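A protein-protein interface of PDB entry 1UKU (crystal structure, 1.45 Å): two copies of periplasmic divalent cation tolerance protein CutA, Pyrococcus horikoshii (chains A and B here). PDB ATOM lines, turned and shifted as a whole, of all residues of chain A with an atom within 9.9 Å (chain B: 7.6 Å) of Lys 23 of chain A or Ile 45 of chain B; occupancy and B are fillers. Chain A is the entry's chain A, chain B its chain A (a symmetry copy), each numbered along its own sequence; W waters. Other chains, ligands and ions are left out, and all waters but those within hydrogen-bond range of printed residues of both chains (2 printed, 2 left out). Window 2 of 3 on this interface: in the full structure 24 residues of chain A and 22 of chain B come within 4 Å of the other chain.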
ATOM      1  N   ALA A  14     -11.261 -19.166 -37.797  1.00  0.00           N
ATOM      2  CA  ALA A  14     -12.104 -18.005 -37.694  1.00  0.00           C
ATOM      3  C   ALA A  14     -13.222 -18.272 -36.674  1.00  0.00           C
ATOM      4  O   ALA A  14     -13.501 -17.432 -35.822  1.00  0.00           O
ATOM      5  CB  ALA A  14     -12.679 -17.687 -39.046  1.00  0.00           C
ATOM      6  N   GLU A  15     -13.887 -19.414 -36.793  1.00  0.00           N
ATOM      7  CA  GLU A  15     -15.013 -19.713 -35.907  1.00  0.00           C
ATOM      8  C   GLU A  15     -14.541 -19.935 -34.475  1.00  0.00           C
ATOM      9  O   GLU A  15     -15.191 -19.466 -33.543  1.00  0.00           O
ATOM     10  CB  GLU A  15     -15.774 -20.955 -36.404  1.00  0.00           C
ATOM     11  CG  GLU A  15     -16.636 -20.673 -37.621  1.00  0.00           C
ATOM     12  CD  GLU A  15     -17.596 -21.790 -37.941  1.00  0.00           C
ATOM     13  OE1 GLU A  15     -17.999 -21.874 -39.126  1.00  0.00           O
ATOM     14  OE2 GLU A  15     -17.995 -22.509 -37.012  1.00  0.00           O
ATOM     15  N   LYS A  16     -13.407 -20.618 -34.280  1.00  0.00           N
ATOM     16  CA  LYS A  16     -12.896 -20.867 -32.936  1.00  0.00           C
ATOM     17  C   LYS A  16     -12.610 -19.548 -32.233  1.00  0.00           C
ATOM     18  O   LYS A  16     -13.015 -19.320 -31.098  1.00  0.00           O
ATOM     19  CB  LYS A  16     -11.610 -21.678 -32.990  1.00  0.00           C
ATOM     20  CG  LYS A  16     -11.028 -21.998 -31.614  1.00  0.00           C
ATOM     21  CD  LYS A  16      -9.853 -22.952 -31.775  1.00  0.00           C
ATOM     22  CE  LYS A  16      -8.890 -22.893 -30.614  1.00  0.00           C
ATOM     23  NZ  LYS A  16      -7.698 -23.743 -30.890  1.00  0.00           N
ATOM     24  N   VAL A  17     -11.922 -18.653 -32.940  1.00  0.00           N
ATOM     25  CA  VAL A  17     -11.525 -17.374 -32.364  1.00  0.00           C
ATOM     26  C   VAL A  17     -12.757 -16.534 -32.083  1.00  0.00           C
ATOM     27  O   VAL A  17     -12.910 -16.011 -31.004  1.00  0.00           O
ATOM     28  CB  VAL A  17     -10.490 -16.657 -33.242  1.00  0.00           C
ATOM     29  CG1 VAL A  17     -10.208 -15.239 -32.721  1.00  0.00           C
ATOM     30  CG2 VAL A  17      -9.190 -17.477 -33.278  1.00  0.00           C
ATOM     31  N   VAL A  18     -13.680 -16.453 -33.032  1.00  0.00           N
ATOM     32  CA  VAL A  18     -14.884 -15.636 -32.842  1.00  0.00           C
ATOM     33  C   VAL A  18     -15.763 -16.152 -31.716  1.00  0.00           C
ATOM     34  O   VAL A  18     -16.282 -15.358 -30.904  1.00  0.00           O
ATOM     35  CB  VAL A  18     -15.675 -15.520 -34.152  1.00  0.00           C
ATOM     36  CG1 VAL A  18     -17.132 -15.132 -33.949  1.00  0.00           C
ATOM     37  CG2 VAL A  18     -14.946 -14.556 -35.083  1.00  0.00           C
ATOM     38  N   LYS A  19     -15.901 -17.461 -31.638  1.00  0.00           N
ATOM     39  CA  LYS A  19     -16.709 -18.038 -30.564  1.00  0.00           C
ATOM     40  C   LYS A  19     -16.022 -17.787 -29.192  1.00  0.00           C
ATOM     41  O   LYS A  19     -16.713 -17.495 -28.219  1.00  0.00           O
ATOM     42  CB  LYS A  19     -16.993 -19.531 -30.789  1.00  0.00           C
ATOM     43  CG  LYS A  19     -17.913 -19.812 -31.956  1.00  0.00           C
ATOM     44  CD  LYS A  19     -18.236 -21.290 -32.142  1.00  0.00           C
ATOM     45  CE  LYS A  19     -19.143 -21.500 -33.342  1.00  0.00           C
ATOM     46  NZ  LYS A  19     -19.478 -22.941 -33.538  1.00  0.00           N
ATOM     47  N   THR A  20     -14.693 -17.861 -29.109  1.00  0.00           N
ATOM     48  CA  THR A  20     -13.973 -17.517 -27.864  1.00  0.00           C
ATOM     49  C   THR A  20     -14.219 -16.050 -27.488  1.00  0.00           C
ATOM     50  O   THR A  20     -14.418 -15.726 -26.327  1.00  0.00           O
ATOM     51  CB  THR A  20     -12.484 -17.771 -28.031  1.00  0.00           C
ATOM     52  OG1 THR A  20     -12.283 -19.167 -28.325  1.00  0.00           O
ATOM     53  CG2 THR A  20     -11.749 -17.484 -26.771  1.00  0.00           C
ATOM     54  N   LEU A  21     -14.211 -15.157 -28.470  1.00  0.00           N
ATOM     55  CA  LEU A  21     -14.388 -13.735 -28.210  1.00  0.00           C
ATOM     56  C   LEU A  21     -15.814 -13.499 -27.737  1.00  0.00           C
ATOM     57  O   LEU A  21     -16.028 -12.652 -26.852  1.00  0.00           O
ATOM     58  CB  LEU A  21     -14.067 -12.891 -29.434  1.00  0.00           C
ATOM     59  CG  LEU A  21     -12.614 -12.890 -29.908  1.00  0.00           C
ATOM     60  CD1 LEU A  21     -12.497 -12.103 -31.239  1.00  0.00           C
ATOM     61  CD2 LEU A  21     -11.603 -12.344 -28.890  1.00  0.00           C
ATOM     62  N   LEU A  22     -16.796 -14.213 -28.296  1.00  0.00           N
ATOM     63  CA  LEU A  22     -18.180 -14.113 -27.829  1.00  0.00           C
ATOM     64  C   LEU A  22     -18.285 -14.627 -26.390  1.00  0.00           C
ATOM     65  O   LEU A  22     -18.899 -13.985 -25.544  1.00  0.00           O
ATOM     66  CB  LEU A  22     -19.145 -14.870 -28.751  1.00  0.00           C
ATOM     67  CG  LEU A  22     -19.429 -14.144 -30.076  1.00  0.00           C
ATOM     68  CD1 LEU A  22     -19.990 -15.110 -31.105  1.00  0.00           C
ATOM     69  CD2 LEU A  22     -20.388 -12.991 -29.883  1.00  0.00           C
ATOM     70  N   LYS A  23     -17.677 -15.768 -26.118  1.00  0.00           N
ATOM     71  CA  LYS A  23     -17.721 -16.338 -24.758  1.00  0.00           C
ATOM     72  C   LYS A  23     -17.125 -15.382 -23.732  1.00  0.00           C
ATOM     73  O   LYS A  23     -17.609 -15.309 -22.593  1.00  0.00           O
ATOM     74  CB  LYS A  23     -17.011 -17.679 -24.711  1.00  0.00           C
ATOM     75  CG  LYS A  23     -17.841 -18.779 -25.413  1.00  0.00           C
ATOM     76  CD  LYS A  23     -17.300 -20.180 -25.222  1.00  0.00           C
ATOM     77  CE  LYS A  23     -15.801 -20.294 -25.391  1.00  0.00           C
ATOM     78  NZ  LYS A  23     -15.392 -21.715 -25.600  1.00  0.00           N
ATOM     79  N   GLU A  24     -16.075 -14.648 -24.122  1.00  0.00           N
ATOM     80  CA  GLU A  24     -15.399 -13.682 -23.276  1.00  0.00           C
ATOM     81  C   GLU A  24     -16.086 -12.346 -23.266  1.00  0.00           C
ATOM     82  O   GLU A  24     -15.623 -11.421 -22.605  1.00  0.00           O
ATOM     83  CB  GLU A  24     -13.930 -13.574 -23.680  1.00  0.00           C
ATOM     84  CG  GLU A  24     -13.199 -14.847 -23.332  1.00  0.00           C
ATOM     85  CD  GLU A  24     -11.748 -14.857 -23.717  1.00  0.00           C
ATOM     86  OE1 GLU A  24     -11.166 -15.961 -23.745  1.00  0.00           O
ATOM     87  OE2 GLU A  24     -11.197 -13.773 -23.977  1.00  0.00           O
ATOM     88  N   ARG A  25     -17.182 -12.242 -24.027  1.00  0.00           N
ATOM     89  CA  ARG A  25     -18.063 -11.086 -24.067  1.00  0.00           C
ATOM     90  C   ARG A  25     -17.328  -9.818 -24.565  1.00  0.00           C
ATOM     91  O   ARG A  25     -17.671  -8.688 -24.270  1.00  0.00           O
ATOM     92  CB  ARG A  25     -18.803 -10.983 -22.720  1.00  0.00           C
ATOM     93  CG  ARG A  25     -19.843 -12.141 -22.565  1.00  0.00           C
ATOM     94  CD  ARG A  25     -21.147 -11.800 -23.148  1.00  0.00           C
ATOM     95  NE  ARG A  25     -22.200 -12.819 -23.035  1.00  0.00           N
ATOM     96  CZ  ARG A  25     -23.435 -12.659 -23.508  1.00  0.00           C
ATOM     97  NH1 ARG A  25     -23.755 -11.559 -24.151  1.00  0.00           N
ATOM     98  NH2 ARG A  25     -24.359 -13.619 -23.389  1.00  0.00           N
ATOM     99  N   LEU A  26     -16.343 -10.052 -25.441  1.00  0.00           N
ATOM    100  CA  LEU A  26     -15.541  -8.972 -25.993  1.00  0.00           C
ATOM    101  C   LEU A  26     -16.107  -8.386 -27.276  1.00  0.00           C
ATOM    102  O   LEU A  26     -15.689  -7.302 -27.669  1.00  0.00           O
ATOM    103  CB  LEU A  26     -14.091  -9.389 -26.215  1.00  0.00           C
ATOM    104  CG  LEU A  26     -13.343  -9.610 -24.904  1.00  0.00           C
ATOM    105  CD1 LEU A  26     -11.992 -10.245 -25.190  1.00  0.00           C
ATOM    106  CD2 LEU A  26     -13.174  -8.299 -24.154  1.00  0.00           C
ATOM    107  N   ILE A  27     -16.992  -9.144 -27.914  1.00  0.00           N
ATOM    108  CA  ILE A  27     -17.719  -8.709 -29.117  1.00  0.00           C
ATOM    109  C   ILE A  27     -19.169  -9.084 -28.956  1.00  0.00           C
ATOM    110  O   ILE A  27     -19.467 -10.045 -28.270  1.00  0.00           O
ATOM    111  CB  ILE A  27     -17.136  -9.305 -30.444  1.00  0.00           C
ATOM    112  CG1 ILE A  27     -17.320 -10.817 -30.549  1.00  0.00           C
ATOM    113  CG2 ILE A  27     -15.679  -8.904 -30.595  1.00  0.00           C
ATOM    114  CD1 ILE A  27     -16.802 -11.392 -31.873  1.00  0.00           C
ATOM    115  N   ALA A  28     -20.045  -8.331 -29.622  1.00  0.00           N
ATOM    116  CA  ALA A  28     -21.459  -8.677 -29.661  1.00  0.00           C
ATOM    117  C   ALA A  28     -21.819  -9.581 -30.827  1.00  0.00           C
ATOM    118  O   ALA A  28     -22.786 -10.335 -30.761  1.00  0.00           O
ATOM    119  CB  ALA A  28     -22.309  -7.437 -29.722  1.00  0.00           C
ATOM    120  N   CYS A  29     -21.065  -9.473 -31.913  1.00  0.00           N
ATOM    121  CA  CYS A  29     -21.339 -10.307 -33.067  1.00  0.00           C
ATOM    122  C   CYS A  29     -20.207 -10.242 -34.052  1.00  0.00           C
ATOM    123  O   CYS A  29     -19.342  -9.368 -33.998  1.00  0.00           O
ATOM    124  CB  CYS A  29     -22.627  -9.885 -33.702  1.00  0.00           C
ATOM    125  SG  CYS A  29     -22.506  -8.304 -34.329  1.00  0.00           S
ATOM    126  N   ALA A  30     -20.191 -11.245 -34.925  1.00  0.00           N
ATOM    127  CA  ALA A  30     -19.225 -11.396 -35.998  1.00  0.00           C
ATOM    128  C   ALA A  30     -19.950 -11.770 -37.297  1.00  0.00           C
ATOM    129  O   ALA A  30     -20.944 -12.480 -37.263  1.00  0.00           O
ATOM    130  CB  ALA A  30     -18.224 -12.409 -35.644  1.00  0.00           C
ATOM    131  N   LEU A  32     -18.750 -13.418 -40.927  1.00  0.00           N
ATOM    132  CA  LEU A  32     -17.617 -14.109 -41.556  1.00  0.00           C
ATOM    133  C   LEU A  32     -17.941 -14.405 -42.993  1.00  0.00           C
ATOM    134  O   LEU A  32     -19.003 -14.917 -43.293  1.00  0.00           O
ATOM    135  CB  LEU A  32     -17.309 -15.423 -40.856  1.00  0.00           C
ATOM    136  CG  LEU A  32     -16.555 -15.327 -39.513  1.00  0.00           C
ATOM    137  CD1 LEU A  32     -17.119 -14.336 -38.508  1.00  0.00           C
ATOM    138  CD2 LEU A  32     -16.419 -16.722 -38.909  1.00  0.00           C
ATOM    139  N   LEU A  65      -9.778  -6.153 -26.646  1.00  0.00           N
ATOM    140  CA  LEU A  65     -10.125  -7.025 -27.761  1.00  0.00           C
ATOM    141  C   LEU A  65      -8.913  -7.236 -28.667  1.00  0.00           C
ATOM    142  O   LEU A  65      -8.638  -8.341 -29.108  1.00  0.00           O
ATOM    143  CB  LEU A  65     -11.287  -6.434 -28.554  1.00  0.00           C
ATOM    144  CG  LEU A  65     -11.635  -7.162 -29.861  1.00  0.00           C
ATOM    145  CD1 LEU A  65     -11.980  -8.607 -29.608  1.00  0.00           C
ATOM    146  CD2 LEU A  65     -12.738  -6.442 -30.591  1.00  0.00           C
ATOM    147  N   ARG A  68      -6.585  -9.685 -27.069  1.00  0.00           N
ATOM    148  CA  ARG A  68      -7.077 -11.045 -27.158  1.00  0.00           C
ATOM    149  C   ARG A  68      -6.965 -11.610 -28.578  1.00  0.00           C
ATOM    150  O   ARG A  68      -6.597 -12.776 -28.759  1.00  0.00           O
ATOM    151  CB  ARG A  68      -8.492 -11.172 -26.608  1.00  0.00           C
ATOM    152  CG  ARG A  68      -8.546 -11.262 -25.117  1.00  0.00           C
ATOM    153  CD  ARG A  68      -7.755 -12.450 -24.530  1.00  0.00           C
ATOM    154  NE  ARG A  68      -8.421 -13.750 -24.564  1.00  0.00           N
ATOM    155  CZ  ARG A  68      -7.814 -14.926 -24.752  1.00  0.00           C
ATOM    156  NH1 ARG A  68      -6.513 -15.001 -24.990  1.00  0.00           N
ATOM    157  NH2 ARG A  68      -8.511 -16.040 -24.703  1.00  0.00           N
ATOM    158  N   LEU A  72      -4.975 -14.957 -29.752  1.00  0.00           N
ATOM    159  CA  LEU A  72      -5.712 -16.089 -30.326  1.00  0.00           C
ATOM    160  C   LEU A  72      -5.424 -16.345 -31.814  1.00  0.00           C
ATOM    161  O   LEU A  72      -5.781 -17.404 -32.346  1.00  0.00           O
ATOM    162  CB  LEU A  72      -7.215 -15.882 -30.155  1.00  0.00           C
ATOM    163  CG  LEU A  72      -7.679 -15.934 -28.706  1.00  0.00           C
ATOM    164  CD1 LEU A  72      -9.132 -15.468 -28.612  1.00  0.00           C
ATOM    165  CD2 LEU A  72      -7.563 -17.329 -28.140  1.00  0.00           C
ATOM    166  N   GLU A  99     -24.967  -6.980 -24.634  1.00  0.00           N
ATOM    167  CA  GLU A  99     -24.333  -8.272 -24.914  1.00  0.00           C
ATOM    168  C   GLU A  99     -22.828  -8.296 -24.695  1.00  0.00           C
ATOM    169  O   GLU A  99     -22.209  -9.348 -24.800  1.00  0.00           O
ATOM    170  CB  GLU A  99     -24.649  -8.694 -26.354  1.00  0.00           C
ATOM    171  CG  GLU A  99     -26.134  -8.942 -26.635  1.00  0.00           C
ATOM    172  CD  GLU A  99     -26.780 -10.124 -25.885  1.00  0.00           C
ATOM    173  OE1 GLU A  99     -28.008 -10.275 -26.077  1.00  0.00           O
ATOM    174  OE2 GLU A  99     -26.156 -10.897 -25.097  1.00  0.00           O
ATOM    175  N   THR A 100     -22.223  -7.167 -24.361  1.00  0.00           N
ATOM    176  CA  THR A 100     -20.782  -7.136 -24.154  1.00  0.00           C
ATOM    177  C   THR A 100     -20.456  -6.946 -22.664  1.00  0.00           C
ATOM    178  O   THR A 100     -21.289  -6.445 -21.897  1.00  0.00           O
ATOM    179  CB  THR A 100     -20.121  -6.062 -25.024  1.00  0.00           C
ATOM    180  OG1 THR A 100     -20.863  -4.834 -25.008  1.00  0.00           O
ATOM    181  CG2 THR A 100     -20.123  -6.535 -26.497  1.00  0.00           C
ATOM    182  N   LYS A 101     -19.244  -7.309 -22.288  1.00  0.00           N
ATOM    183  CA  LYS A 101     -18.862  -7.453 -20.892  1.00  0.00           C
ATOM    184  C   LYS A 101     -18.846  -6.114 -20.179  1.00  0.00           C
ATOM    185  O   LYS A 101     -18.632  -5.058 -20.782  1.00  0.00           O
ATOM    186  CB  LYS A 101     -17.519  -8.161 -20.751  1.00  0.00           C
ATOM    187  CG  LYS A 101     -16.341  -7.328 -21.185  1.00  0.00           C
ATOM    188  CD  LYS A 101     -15.013  -8.090 -21.051  1.00  0.00           C
ATOM    189  CE  LYS A 101     -14.469  -8.103 -19.638  1.00  0.00           C
ATOM    190  NZ  LYS A 101     -13.164  -8.859 -19.522  1.00  0.00           N
ATOM    191  N   ALA B  37     -23.185 -15.229 -39.672  1.00  0.00           N
ATOM    192  CA  ALA B  37     -23.190 -14.396 -38.477  1.00  0.00           C
ATOM    193  C   ALA B  37     -23.143 -15.268 -37.216  1.00  0.00           C
ATOM    194  O   ALA B  37     -23.778 -16.290 -37.163  1.00  0.00           O
ATOM    195  CB  ALA B  37     -24.409 -13.516 -38.431  1.00  0.00           C
ATOM    196  N   PHE B  38     -22.399 -14.828 -36.222  1.00  0.00           N
ATOM    197  CA  PHE B  38     -22.293 -15.463 -34.932  1.00  0.00           C
ATOM    198  C   PHE B  38     -22.549 -14.436 -33.865  1.00  0.00           C
ATOM    199  O   PHE B  38     -22.003 -13.331 -33.901  1.00  0.00           O
ATOM    200  CB  PHE B  38     -20.921 -16.084 -34.738  1.00  0.00           C
ATOM    201  CG  PHE B  38     -20.615 -17.162 -35.720  1.00  0.00           C
ATOM    202  CD1 PHE B  38     -20.158 -16.856 -36.987  1.00  0.00           C
ATOM    203  CD2 PHE B  38     -20.802 -18.478 -35.383  1.00  0.00           C
ATOM    204  CE1 PHE B  38     -19.922 -17.836 -37.909  1.00  0.00           C
ATOM    205  CE2 PHE B  38     -20.549 -19.485 -36.323  1.00  0.00           C
ATOM    206  CZ  PHE B  38     -20.108 -19.138 -37.580  1.00  0.00           C
ATOM    207  N   TYR B  39     -23.429 -14.767 -32.919  1.00  0.00           N
ATOM    208  CA  TYR B  39     -23.799 -13.815 -31.883  1.00  0.00           C
ATOM    209  C   TYR B  39     -24.466 -14.591 -30.749  1.00  0.00           C
ATOM    210  O   TYR B  39     -24.643 -15.794 -30.843  1.00  0.00           O
ATOM    211  CB  TYR B  39     -24.705 -12.720 -32.444  1.00  0.00           C
ATOM    212  CG  TYR B  39     -25.914 -13.265 -33.150  1.00  0.00           C
ATOM    213  CD1 TYR B  39     -25.879 -13.517 -34.501  1.00  0.00           C
ATOM    214  CD2 TYR B  39     -27.083 -13.567 -32.450  1.00  0.00           C
ATOM    215  CE1 TYR B  39     -26.964 -14.046 -35.153  1.00  0.00           C
ATOM    216  CE2 TYR B  39     -28.181 -14.086 -33.097  1.00  0.00           C
ATOM    217  CZ  TYR B  39     -28.100 -14.337 -34.444  1.00  0.00           C
ATOM    218  OH  TYR B  39     -29.194 -14.862 -35.109  1.00  0.00           O
ATOM    219  N   TRP B  40     -24.782 -13.899 -29.655  1.00  0.00           N
ATOM    220  CA  TRP B  40     -25.450 -14.506 -28.504  1.00  0.00           C
ATOM    221  C   TRP B  40     -26.945 -14.422 -28.645  1.00  0.00           C
ATOM    222  O   TRP B  40     -27.472 -13.378 -29.012  1.00  0.00           O
ATOM    223  CB  TRP B  40     -25.124 -13.774 -27.206  1.00  0.00           C
ATOM    224  CG  TRP B  40     -23.795 -14.046 -26.685  1.00  0.00           C
ATOM    225  CD1 TRP B  40     -22.701 -13.239 -26.787  1.00  0.00           C
ATOM    226  CD2 TRP B  40     -23.371 -15.228 -25.994  1.00  0.00           C
ATOM    227  NE1 TRP B  40     -21.627 -13.838 -26.178  1.00  0.00           N
ATOM    228  CE2 TRP B  40     -21.999 -15.070 -25.701  1.00  0.00           C
ATOM    229  CE3 TRP B  40     -24.005 -16.409 -25.606  1.00  0.00           C
ATOM    230  CZ2 TRP B  40     -21.262 -16.038 -25.007  1.00  0.00           C
ATOM    231  CZ3 TRP B  40     -23.269 -17.383 -24.914  1.00  0.00           C
ATOM    232  CH2 TRP B  40     -21.914 -17.190 -24.630  1.00  0.00           C
ATOM    233  N   TRP B  41     -27.598 -15.550 -28.369  1.00  0.00           N
ATOM    234  CA  TRP B  41     -29.039 -15.593 -28.151  1.00  0.00           C
ATOM    235  C   TRP B  41     -29.307 -16.461 -26.937  1.00  0.00           C
ATOM    236  O   TRP B  41     -28.991 -17.631 -26.945  1.00  0.00           O
ATOM    237  CB  TRP B  41     -29.728 -16.162 -29.376  1.00  0.00           C
ATOM    238  CG  TRP B  41     -31.176 -16.346 -29.193  1.00  0.00           C
ATOM    239  CD1 TRP B  41     -32.118 -15.375 -29.068  1.00  0.00           C
ATOM    240  CD2 TRP B  41     -31.863 -17.595 -29.089  1.00  0.00           C
ATOM    241  NE1 TRP B  41     -33.362 -15.942 -28.899  1.00  0.00           N
ATOM    242  CE2 TRP B  41     -33.230 -17.305 -28.901  1.00  0.00           C
ATOM    243  CE3 TRP B  41     -31.461 -18.938 -29.131  1.00  0.00           C
ATOM    244  CZ2 TRP B  41     -34.200 -18.313 -28.765  1.00  0.00           C
ATOM    245  CZ3 TRP B  41     -32.426 -19.934 -28.993  1.00  0.00           C
ATOM    246  CH2 TRP B  41     -33.771 -19.614 -28.815  1.00  0.00           C
ATOM    247  N   GLU B  42     -29.838 -15.852 -25.880  1.00  0.00           N
ATOM    248  CA  GLU B  42     -30.317 -16.565 -24.692  1.00  0.00           C
ATOM    249  C   GLU B  42     -29.273 -17.546 -24.140  1.00  0.00           C
ATOM    250  O   GLU B  42     -29.532 -18.729 -23.937  1.00  0.00           O
ATOM    251  CB  GLU B  42     -31.651 -17.243 -25.001  1.00  0.00           C
ATOM    252  CG  GLU B  42     -32.762 -16.255 -25.317  1.00  0.00           C
ATOM    253  CD  GLU B  42     -34.124 -16.905 -25.560  1.00  0.00           C
ATOM    254  OE1 GLU B  42     -35.102 -16.146 -25.775  1.00  0.00           O
ATOM    255  OE2 GLU B  42     -34.233 -18.151 -25.567  1.00  0.00           O
ATOM    256  N   GLY B  43     -28.061 -17.043 -23.924  1.00  0.00           N
ATOM    257  CA  GLY B  43     -27.018 -17.798 -23.257  1.00  0.00           C
ATOM    258  C   GLY B  43     -26.315 -18.815 -24.134  1.00  0.00           C
ATOM    259  O   GLY B  43     -25.544 -19.637 -23.640  1.00  0.00           O
ATOM    260  N   LYS B  44     -26.600 -18.769 -25.441  1.00  0.00           N
ATOM    261  CA  LYS B  44     -26.026 -19.698 -26.408  1.00  0.00           C
ATOM    262  C   LYS B  44     -25.409 -18.918 -27.573  1.00  0.00           C
ATOM    263  O   LYS B  44     -25.941 -17.882 -27.966  1.00  0.00           O
ATOM    264  CB  LYS B  44     -27.097 -20.613 -26.966  1.00  0.00           C
ATOM    265  CG  LYS B  44     -27.721 -21.592 -25.954  1.00  0.00           C
ATOM    266  CD  LYS B  44     -29.036 -22.169 -26.490  1.00  0.00           C
ATOM    267  CE  LYS B  44     -30.191 -21.163 -26.405  1.00  0.00           C
ATOM    268  NZ  LYS B  44     -30.591 -20.868 -25.008  1.00  0.00           N
ATOM    269  N   ILE B  45     -24.335 -19.435 -28.153  1.00  0.00           N
ATOM    270  CA  ILE B  45     -23.813 -18.852 -29.382  1.00  0.00           C
ATOM    271  C   ILE B  45     -24.649 -19.388 -30.537  1.00  0.00           C
ATOM    272  O   ILE B  45     -24.786 -20.599 -30.724  1.00  0.00           O
ATOM    273  CB  ILE B  45     -22.314 -19.102 -29.540  1.00  0.00           C
ATOM    274  CG1 ILE B  45     -21.588 -18.321 -28.440  1.00  0.00           C
ATOM    275  CG2 ILE B  45     -21.850 -18.623 -30.923  1.00  0.00           C
ATOM    276  CD1 ILE B  45     -20.096 -18.593 -28.310  1.00  0.00           C
ATOM    277  N   GLU B  46     -25.237 -18.463 -31.263  1.00  0.00           N
ATOM    278  CA  GLU B  46     -26.113 -18.722 -32.375  1.00  0.00           C
ATOM    279  C   GLU B  46     -25.364 -18.365 -33.652  1.00  0.00           C
ATOM    280  O   GLU B  46     -24.584 -17.411 -33.681  1.00  0.00           O
ATOM    281  CB  GLU B  46     -27.367 -17.834 -32.262  1.00  0.00           C
ATOM    282  CG  GLU B  46     -28.341 -17.917 -33.438  1.00  0.00           C
ATOM    283  CD  GLU B  46     -29.765 -17.512 -33.073  1.00  0.00           C
ATOM    284  OE1 GLU B  46     -30.241 -16.458 -33.549  1.00  0.00           O
ATOM    285  OE2 GLU B  46     -30.411 -18.236 -32.303  1.00  0.00           O
ATOM    286  N   GLU B  47     -25.597 -19.141 -34.686  1.00  0.00           N
ATOM    287  CA  GLU B  47     -25.197 -18.782 -36.036  1.00  0.00           C
ATOM    288  C   GLU B  47     -26.424 -18.594 -36.887  1.00  0.00           C
ATOM    289  O   GLU B  47     -27.426 -19.296 -36.728  1.00  0.00           O
ATOM    290  CB  GLU B  47     -24.326 -19.868 -36.632  1.00  0.00           C
ATOM    291  CG  GLU B  47     -23.857 -19.614 -38.073  1.00  0.00           C
ATOM    292  CD  GLU B  47     -23.139 -20.778 -38.672  1.00  0.00           C
ATOM    293  OE1 GLU B  47     -23.097 -21.881 -38.081  1.00  0.00           O
ATOM    294  OE2 GLU B  47     -22.578 -20.599 -39.786  1.00  0.00           O
HETATM  295  O   HOH W   1     -22.083 -22.554 -35.121  1.00  0.00           O
HETATM  296  O   HOH W   2     -24.291 -11.136 -28.949  1.00  0.00           O
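N of Ala 30 of chain A is in hydrogen-bond range of O of Phe 38 of chain B, at 2.9 Å.
NE of Arg 25 of chain A sits close to NE1 of Trp 40 of chain B (3.4 Å).
The backbone carbonyl oxygen of Leu 22 of chain A is in hydrogen-bond range of the indole nitrogen of Trp 40 of chain B, at 2.8 Å.
The backbone carbonyl oxygen of Arg 25 of chain A sits at hydrogen-bond distance from the backbone NH of Lys 101 of chain A (2.9 Å).
OH of Tyr 39 of chain B is in hydrogen-bond range of OE1 of Glu 46 of chain B, at 2.5 Å.
The side-chain carboxylate (OE2) of Glu 99 of chain A is in salt-bridge range of the guanidinium group (NH1) of Arg 25 of chain A (2.7 Å).
The side-chain carboxylate (OE2) of Glu 15 of chain A lies within salt-bridge range of the side-chain amino group (NZ) of Lys 19 of chain A, at 3.8 Å.
Phe 38 of chain B touches Val 18 of chain A (CB to CG1, 3.99 Å).
Phe 38 of chain B touches Lys 19 of chain A.
Phe 38 of chain B touches Leu 22 of chain A (C to CD1, 3.8 Å).
Leu 22 of chain A touches Tyr 39 of chain B (CD1 to N, 3.9 Å).
Leu 22 of chain A touches Ile 45 of chain B (CB to CD1, 3.9 Å).
CA of Lys 23 of chain A touches CZ2 of Trp 40 of chain B (3.6 Å).
Cys 29 of chain A touches Phe 38 of chain B (CA to O, 3.2 Å).
Cys 29 of chain A touches Tyr 39 of chain B.
O of Ala 30 of chain A touches CA of Ala 37 of chain B (3.2 Å).
CD2 of Leu 32 of chain A touches CE1 of Phe 38 of chain B (3.8 Å).
Lys 23 of chain A touches just these residues of chain B: Trp 40 (3.6 Å) and Ile 45 (3.7 Å).
Of the printed residues of chain B, Cys 29 of chain A touches Phe 38 and Tyr 39.
Printed residues of chain B within 4 Å of Glu 15 of chain A: Phe 38 (3.7 Å).
Of the printed residues of chain B, Lys 19 of chain A touches Phe 38 and Ile 45.
Of the printed residues of chain A, Ala 37 of chain B touches Ala 30.
Of the 24 printed residues of chain A, 11 touch a printed residue of chain B.
Printed residues of chain A that touch a printed residue of chain B: Glu 15, Val 18, Lys 19, Leu 22, Lys 23, Arg 25, Ala 28, Cys 29, Ala 30, Leu 32 and Glu 99.
Of the 11 printed residues of chain B, 5 touch a printed residue of chain A.
Among the printed residues, no Asp or Glu carboxylate lies within 4 Å of a Lys or Arg side-chain nitrogen of the other chain.
No position is printed for both chains.
Of the 18 pairs that touch across the chains among the printed residues, none has its exchanged pair printed and touching as well.
Water W2 bridges the backbone carbonyl oxygen (O) of Ala 28 of chain A and the backbone NH (N) of Trp 40 of chain B.
Water W1 bridges NZ of Lys 19 of chain A (3.1 Å) and OE1 of Glu 47 of chain B (3.2 Å).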
